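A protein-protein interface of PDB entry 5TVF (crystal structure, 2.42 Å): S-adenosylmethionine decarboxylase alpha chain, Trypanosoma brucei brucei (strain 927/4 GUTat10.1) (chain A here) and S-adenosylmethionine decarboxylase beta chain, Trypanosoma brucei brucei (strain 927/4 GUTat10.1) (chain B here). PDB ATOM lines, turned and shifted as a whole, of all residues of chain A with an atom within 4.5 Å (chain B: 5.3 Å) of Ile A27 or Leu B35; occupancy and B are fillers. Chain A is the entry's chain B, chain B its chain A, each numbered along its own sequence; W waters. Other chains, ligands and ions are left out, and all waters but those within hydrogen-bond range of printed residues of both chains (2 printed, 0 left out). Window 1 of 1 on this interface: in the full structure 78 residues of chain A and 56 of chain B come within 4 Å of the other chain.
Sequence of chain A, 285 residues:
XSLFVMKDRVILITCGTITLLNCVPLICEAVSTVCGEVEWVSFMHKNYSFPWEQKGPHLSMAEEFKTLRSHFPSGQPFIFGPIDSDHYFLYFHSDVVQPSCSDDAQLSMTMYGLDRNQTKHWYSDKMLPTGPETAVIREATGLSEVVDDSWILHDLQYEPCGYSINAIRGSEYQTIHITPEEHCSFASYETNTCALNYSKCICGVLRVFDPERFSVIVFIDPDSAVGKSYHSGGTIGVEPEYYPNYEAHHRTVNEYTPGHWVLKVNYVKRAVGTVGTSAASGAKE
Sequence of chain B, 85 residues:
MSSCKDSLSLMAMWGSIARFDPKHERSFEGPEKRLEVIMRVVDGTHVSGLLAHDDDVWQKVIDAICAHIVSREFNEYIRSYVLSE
The backbone carbonyl oxygen (O) of Leu B35 is in hydrogen-bond range of the backbone NH (N) of Leu A12 (2.8 Å). The backbone NH of Ser A42 sits at hydrogen-bond distance from the backbone carbonyl oxygen of Glu B36 (3.0 Å). The backbone carbonyl oxygen of Val B37 lies within hydrogen-bond range of the backbone NH of Val A10 (2.9 Å).
The guanidinium group (NH1) of Arg B34 is in salt-bridge range of the side-chain carboxylate (OE1) of Glu B36 (2.8 Å). The side-chain sulfur (SG) of Cys A23 sits at hydrogen-bond distance from the backbone carbonyl oxygen (O) of Leu A20, at 3.4 Å.
Val A24 touches none of the printed residues of chain B. Of the printed residues of chain B, Ser A42 touches Arg B34 (3.7 Å), Leu B35 (3.5 Å) and Glu B36 (3.0 Å). Of the printed residues of chain B, Phe A43 touches Arg B34 (3.4 Å). Of chain A, only Val A10, Ile A11, Leu A12, Leu A20, Ile A27 and Ser A42 come within 4 Å of Leu B35. Of the printed residues of chain A, Val B37 touches Val A10 and Ile A27. Of the printed residues of chain A, Val B61 touches Cys A23 (3.7 Å) and Leu A26 (3.9 Å). The nearest printed residue of chain A that does not touch Leu B35 is Val A24 (4.1 Å). The nearest printed residue of chain B that does not touch Ile A11 is Val B37 (5.3 Å).
Of the 16 printed residues of chain A, 10 touch a printed residue of chain B. Hydrophobic or aromatic side chains of chain A within 4 Å of the printed part of chain B: Ile A11, Leu A20, Leu A26, Ile A27, Val A41 and Phe A43. Hydrophobic or aromatic side chains of chain B within 4 Å of the printed part of chain A: Leu B35, Val B37 and Val B61.
Water W2 bridges the side-chain hydroxyl of Ser A42 (2.4 Å) and the side-chain carboxylate of Glu B36 (2.7 Å). Water W1 bridges the side-chain hydroxyl (OG) of Ser A42 (2.8 Å) and the guanidinium group (NH1) of Arg B34 (3.0 Å).
Val A10 touches Glu B36. CD1 of Ile A11 touches NH2 of Arg B34, at 3.6 Å. Leu B35 touches Ile A11. CG1 of Ile A11 touches CG of Glu B36, at 3.8 Å. CB of Lys B33 touches CD2 of Leu A20, 3.7 Å away. CD2 of Leu A20 touches CB of Leu B35, 3.7 Å away. CG1 of Val B61 touches CB of Cys A23, 3.7 Å away. Val B61 touches Leu A26 (CG2 to CB, 3.9 Å). Ile A27 touches Val B37. O of Ser A42 touches CA of Leu B35, 3.5 Å away.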
ATOM      1  N   VAL A  10       4.274 -31.647   2.099  1.00  0.00           N
ATOM      2  CA  VAL A  10       4.998 -31.145   0.939  1.00  0.00           C
ATOM      3  C   VAL A  10       5.384 -29.703   1.226  1.00  0.00           C
ATOM      4  O   VAL A  10       4.635 -28.970   1.880  1.00  0.00           O
ATOM      5  CB  VAL A  10       4.154 -31.237  -0.353  1.00  0.00           C
ATOM      6  CG1 VAL A  10       4.774 -30.404  -1.473  1.00  0.00           C
ATOM      7  CG2 VAL A  10       4.018 -32.685  -0.790  1.00  0.00           C
ATOM      8  N   ILE A  11       6.554 -29.299   0.743  1.00  0.00           N
ATOM      9  CA  ILE A  11       7.029 -27.924   0.859  1.00  0.00           C
ATOM     10  C   ILE A  11       7.519 -27.514  -0.519  1.00  0.00           C
ATOM     11  O   ILE A  11       8.564 -27.992  -0.980  1.00  0.00           O
ATOM     12  CB  ILE A  11       8.142 -27.772   1.906  1.00  0.00           C
ATOM     13  CG1 ILE A  11       7.594 -28.074   3.304  1.00  0.00           C
ATOM     14  CG2 ILE A  11       8.746 -26.362   1.850  1.00  0.00           C
ATOM     15  CD1 ILE A  11       8.657 -28.126   4.385  1.00  0.00           C
ATOM     16  N   LEU A  12       6.772 -26.636  -1.179  1.00  0.00           N
ATOM     17  CA  LEU A  12       7.087 -26.199  -2.531  1.00  0.00           C
ATOM     18  C   LEU A  12       7.515 -24.739  -2.484  1.00  0.00           C
ATOM     19  O   LEU A  12       6.735 -23.870  -2.078  1.00  0.00           O
ATOM     20  CB  LEU A  12       5.883 -26.397  -3.455  1.00  0.00           C
ATOM     21  CG  LEU A  12       6.078 -26.157  -4.953  1.00  0.00           C
ATOM     22  CD1 LEU A  12       7.346 -26.814  -5.481  1.00  0.00           C
ATOM     23  CD2 LEU A  12       4.864 -26.677  -5.713  1.00  0.00           C
ATOM     24  N   LEU A  20       2.604 -20.474  -8.406  1.00  0.00           N
ATOM     25  CA  LEU A  20       2.745 -21.623  -7.519  1.00  0.00           C
ATOM     26  C   LEU A  20       1.400 -22.273  -7.212  1.00  0.00           C
ATOM     27  O   LEU A  20       1.300 -23.503  -7.140  1.00  0.00           O
ATOM     28  CB  LEU A  20       3.435 -21.188  -6.226  1.00  0.00           C
ATOM     29  CG  LEU A  20       3.516 -22.230  -5.112  1.00  0.00           C
ATOM     30  CD1 LEU A  20       4.120 -23.516  -5.630  1.00  0.00           C
ATOM     31  CD2 LEU A  20       4.328 -21.701  -3.945  1.00  0.00           C
ATOM     32  N   CYS A  23      -0.795 -25.721  -8.567  1.00  0.00           N
ATOM     33  CA  CYS A  23      -0.579 -27.130  -8.275  1.00  0.00           C
ATOM     34  C   CYS A  23      -1.357 -27.618  -7.058  1.00  0.00           C
ATOM     35  O   CYS A  23      -1.203 -28.781  -6.672  1.00  0.00           O
ATOM     36  CB  CYS A  23       0.913 -27.395  -8.064  1.00  0.00           C
ATOM     37  SG  CYS A  23       1.540 -26.848  -6.463  1.00  0.00           S
ATOM     38  N   VAL A  24      -2.188 -26.768  -6.451  1.00  0.00           N
ATOM     39  CA  VAL A  24      -2.939 -27.187  -5.266  1.00  0.00           C
ATOM     40  C   VAL A  24      -3.852 -28.370  -5.564  1.00  0.00           C
ATOM     41  O   VAL A  24      -3.877 -29.319  -4.764  1.00  0.00           O
ATOM     42  CB  VAL A  24      -3.703 -25.988  -4.676  1.00  0.00           C
ATOM     43  CG1 VAL A  24      -4.604 -26.431  -3.530  1.00  0.00           C
ATOM     44  CG2 VAL A  24      -2.724 -24.925  -4.203  1.00  0.00           C
ATOM     45  N   PRO A  25      -4.621 -28.386  -6.657  1.00  0.00           N
ATOM     46  CA  PRO A  25      -5.486 -29.551  -6.914  1.00  0.00           C
ATOM     47  C   PRO A  25      -4.738 -30.874  -6.940  1.00  0.00           C
ATOM     48  O   PRO A  25      -5.233 -31.867  -6.394  1.00  0.00           O
ATOM     49  CB  PRO A  25      -6.110 -29.220  -8.277  1.00  0.00           C
ATOM     50  CG  PRO A  25      -6.091 -27.738  -8.348  1.00  0.00           C
ATOM     51  CD  PRO A  25      -4.833 -27.315  -7.647  1.00  0.00           C
ATOM     52  N   LEU A  26      -3.555 -30.916  -7.557  1.00  0.00           N
ATOM     53  CA  LEU A  26      -2.805 -32.166  -7.629  1.00  0.00           C
ATOM     54  C   LEU A  26      -2.206 -32.546  -6.280  1.00  0.00           C
ATOM     55  O   LEU A  26      -2.093 -33.738  -5.969  1.00  0.00           O
ATOM     56  CB  LEU A  26      -1.708 -32.059  -8.687  1.00  0.00           C
ATOM     57  CG  LEU A  26      -2.206 -32.089 -10.133  1.00  0.00           C
ATOM     58  CD1 LEU A  26      -1.104 -31.664 -11.090  1.00  0.00           C
ATOM     59  CD2 LEU A  26      -2.726 -33.476 -10.499  1.00  0.00           C
ATOM     60  N   ILE A  27      -1.813 -31.560  -5.469  1.00  0.00           N
ATOM     61  CA  ILE A  27      -1.338 -31.864  -4.122  1.00  0.00           C
ATOM     62  C   ILE A  27      -2.456 -32.499  -3.306  1.00  0.00           C
ATOM     63  O   ILE A  27      -2.252 -33.507  -2.621  1.00  0.00           O
ATOM     64  CB  ILE A  27      -0.790 -30.594  -3.444  1.00  0.00           C
ATOM     65  CG1 ILE A  27       0.462 -30.107  -4.182  1.00  0.00           C
ATOM     66  CG2 ILE A  27      -0.473 -30.866  -1.973  1.00  0.00           C
ATOM     67  CD1 ILE A  27       1.008 -28.783  -3.682  1.00  0.00           C
ATOM     68  N   CYS A  28      -3.656 -31.914  -3.367  1.00  0.00           N
ATOM     69  CA  CYS A  28      -4.803 -32.513  -2.694  1.00  0.00           C
ATOM     70  C   CYS A  28      -5.042 -33.935  -3.185  1.00  0.00           C
ATOM     71  O   CYS A  28      -5.325 -34.837  -2.387  1.00  0.00           O
ATOM     72  CB  CYS A  28      -6.051 -31.657  -2.913  1.00  0.00           C
ATOM     73  SG  CYS A  28      -5.968 -30.005  -2.177  1.00  0.00           S
ATOM     74  N   GLU A  29      -4.929 -34.156  -4.495  1.00  0.00           N
ATOM     75  CA  GLU A  29      -5.069 -35.507  -5.026  1.00  0.00           C
ATOM     76  C   GLU A  29      -3.949 -36.406  -4.520  1.00  0.00           C
ATOM     77  O   GLU A  29      -4.186 -37.567  -4.166  1.00  0.00           O
ATOM     78  CB  GLU A  29      -5.080 -35.472  -6.554  1.00  0.00           C
ATOM     79  CG  GLU A  29      -5.612 -36.746  -7.195  1.00  0.00           C
ATOM     80  CD  GLU A  29      -5.523 -36.723  -8.710  1.00  0.00           C
ATOM     81  OE1 GLU A  29      -4.468 -36.316  -9.241  1.00  0.00           O
ATOM     82  OE2 GLU A  29      -6.511 -37.110  -9.372  1.00  0.00           O
ATOM     83  N   ALA A  30      -2.721 -35.884  -4.470  1.00  0.00           N
ATOM     84  CA  ALA A  30      -1.597 -36.677  -3.983  1.00  0.00           C
ATOM     85  C   ALA A  30      -1.807 -37.119  -2.542  1.00  0.00           C
ATOM     86  O   ALA A  30      -1.268 -38.152  -2.125  1.00  0.00           O
ATOM     87  CB  ALA A  30      -0.300 -35.881  -4.106  1.00  0.00           C
ATOM     88  N   VAL A  31      -2.579 -36.356  -1.769  1.00  0.00           N
ATOM     89  CA  VAL A  31      -2.854 -36.733  -0.388  1.00  0.00           C
ATOM     90  C   VAL A  31      -3.977 -37.762  -0.317  1.00  0.00           C
ATOM     91  O   VAL A  31      -3.970 -38.633   0.562  1.00  0.00           O
ATOM     92  CB  VAL A  31      -3.183 -35.480   0.444  1.00  0.00           C
ATOM     93  CG1 VAL A  31      -3.664 -35.860   1.840  1.00  0.00           C
ATOM     94  CG2 VAL A  31      -1.966 -34.575   0.533  1.00  0.00           C
ATOM     95  N   VAL A  41      -2.498 -26.038   5.838  1.00  0.00           N
ATOM     96  CA  VAL A  41      -2.000 -25.445   4.605  1.00  0.00           C
ATOM     97  C   VAL A  41      -1.560 -24.023   4.911  1.00  0.00           C
ATOM     98  O   VAL A  41      -2.300 -23.261   5.542  1.00  0.00           O
ATOM     99  CB  VAL A  41      -3.061 -25.458   3.490  1.00  0.00           C
ATOM    100  CG1 VAL A  41      -2.523 -24.773   2.235  1.00  0.00           C
ATOM    101  CG2 VAL A  41      -3.486 -26.886   3.186  1.00  0.00           C
ATOM    102  N   SER A  42      -0.359 -23.670   4.464  1.00  0.00           N
ATOM    103  CA  SER A  42       0.158 -22.319   4.602  1.00  0.00           C
ATOM    104  C   SER A  42       0.699 -21.866   3.257  1.00  0.00           C
ATOM    105  O   SER A  42       1.416 -22.615   2.588  1.00  0.00           O
ATOM    106  CB  SER A  42       1.262 -22.245   5.664  1.00  0.00           C
ATOM    107  OG  SER A  42       2.440 -22.902   5.222  1.00  0.00           O
ATOM    108  N   PHE A  43       0.338 -20.651   2.858  1.00  0.00           N
ATOM    109  CA  PHE A  43       0.944 -19.984   1.716  1.00  0.00           C
ATOM    110  C   PHE A  43       1.595 -18.703   2.207  1.00  0.00           C
ATOM    111  O   PHE A  43       0.963 -17.913   2.916  1.00  0.00           O
ATOM    112  CB  PHE A  43      -0.078 -19.672   0.627  1.00  0.00           C
ATOM    113  CG  PHE A  43       0.458 -18.787  -0.455  1.00  0.00           C
ATOM    114  CD1 PHE A  43       1.366 -19.275  -1.378  1.00  0.00           C
ATOM    115  CD2 PHE A  43       0.067 -17.461  -0.540  1.00  0.00           C
ATOM    116  CE1 PHE A  43       1.867 -18.461  -2.372  1.00  0.00           C
ATOM    117  CE2 PHE A  43       0.563 -16.644  -1.535  1.00  0.00           C
ATOM    118  CZ  PHE A  43       1.467 -17.146  -2.450  1.00  0.00           C
ATOM    119  N   LYS B  33       7.848 -17.684  -3.355  1.00  0.00           N
ATOM    120  CA  LYS B  33       6.563 -18.145  -2.855  1.00  0.00           C
ATOM    121  C   LYS B  33       6.761 -19.506  -2.199  1.00  0.00           C
ATOM    122  O   LYS B  33       7.543 -20.330  -2.684  1.00  0.00           O
ATOM    123  CB  LYS B  33       5.540 -18.246  -3.988  1.00  0.00           C
ATOM    124  CG  LYS B  33       5.506 -17.030  -4.905  1.00  0.00           C
ATOM    125  CD  LYS B  33       4.539 -17.232  -6.061  1.00  0.00           C
ATOM    126  CE  LYS B  33       4.559 -16.062  -7.031  1.00  0.00           C
ATOM    127  NZ  LYS B  33       5.903 -15.844  -7.632  1.00  0.00           N
ATOM    128  N   ARG B  34       6.062 -19.732  -1.089  1.00  0.00           N
ATOM    129  CA  ARG B  34       6.212 -20.956  -0.314  1.00  0.00           C
ATOM    130  C   ARG B  34       4.841 -21.556  -0.046  1.00  0.00           C
ATOM    131  O   ARG B  34       3.951 -20.874   0.472  1.00  0.00           O
ATOM    132  CB  ARG B  34       6.939 -20.688   1.008  1.00  0.00           C
ATOM    133  CG  ARG B  34       7.275 -21.944   1.793  1.00  0.00           C
ATOM    134  CD  ARG B  34       7.911 -21.603   3.131  1.00  0.00           C
ATOM    135  NE  ARG B  34       8.388 -22.793   3.830  1.00  0.00           N
ATOM    136  CZ  ARG B  34       7.629 -23.572   4.597  1.00  0.00           C
ATOM    137  NH1 ARG B  34       6.342 -23.297   4.772  1.00  0.00           N
ATOM    138  NH2 ARG B  34       8.162 -24.633   5.190  1.00  0.00           N
ATOM    139  N   LEU B  35       4.679 -22.829  -0.395  1.00  0.00           N
ATOM    140  CA  LEU B  35       3.453 -23.573  -0.147  1.00  0.00           C
ATOM    141  C   LEU B  35       3.785 -24.804   0.684  1.00  0.00           C
ATOM    142  O   LEU B  35       4.710 -25.553   0.347  1.00  0.00           O
ATOM    143  CB  LEU B  35       2.786 -23.987  -1.461  1.00  0.00           C
ATOM    144  CG  LEU B  35       1.477 -24.768  -1.338  1.00  0.00           C
ATOM    145  CD1 LEU B  35       0.385 -23.900  -0.727  1.00  0.00           C
ATOM    146  CD2 LEU B  35       1.049 -25.306  -2.695  1.00  0.00           C
ATOM    147  N   GLU B  36       3.039 -25.009   1.766  1.00  0.00           N
ATOM    148  CA  GLU B  36       3.229 -26.171   2.623  1.00  0.00           C
ATOM    149  C   GLU B  36       1.882 -26.814   2.918  1.00  0.00           C
ATOM    150  O   GLU B  36       0.937 -26.132   3.324  1.00  0.00           O
ATOM    151  CB  GLU B  36       3.934 -25.794   3.930  1.00  0.00           C
ATOM    152  CG  GLU B  36       4.255 -26.995   4.805  1.00  0.00           C
ATOM    153  CD  GLU B  36       5.130 -26.648   5.995  1.00  0.00           C
ATOM    154  OE1 GLU B  36       5.321 -25.445   6.271  1.00  0.00           O
ATOM    155  OE2 GLU B  36       5.629 -27.586   6.651  1.00  0.00           O
ATOM    156  N   VAL B  37       1.804 -28.127   2.712  1.00  0.00           N
ATOM    157  CA  VAL B  37       0.600 -28.906   2.977  1.00  0.00           C
ATOM    158  C   VAL B  37       0.992 -30.074   3.871  1.00  0.00           C
ATOM    159  O   VAL B  37       1.869 -30.866   3.508  1.00  0.00           O
ATOM    160  CB  VAL B  37      -0.057 -29.415   1.682  1.00  0.00           C
ATOM    161  CG1 VAL B  37      -1.323 -30.212   1.999  1.00  0.00           C
ATOM    162  CG2 VAL B  37      -0.375 -28.255   0.751  1.00  0.00           C
ATOM    163  N   VAL B  61       3.054 -32.640 -10.809  1.00  0.00           N
ATOM    164  CA  VAL B  61       2.755 -31.470  -9.990  1.00  0.00           C
ATOM    165  C   VAL B  61       3.563 -30.270 -10.470  1.00  0.00           C
ATOM    166  O   VAL B  61       3.038 -29.158 -10.600  1.00  0.00           O
ATOM    167  CB  VAL B  61       3.025 -31.778  -8.506  1.00  0.00           C
ATOM    168  CG1 VAL B  61       2.890 -30.527  -7.652  1.00  0.00           C
ATOM    169  CG2 VAL B  61       2.073 -32.855  -8.011  1.00  0.00           C
HETATM  170  O   HOH W   1       4.208 -21.654   3.423  1.00  0.00           O
HETATM  171  O   HOH W   2       3.152 -24.128   7.220  1.00  0.00           O
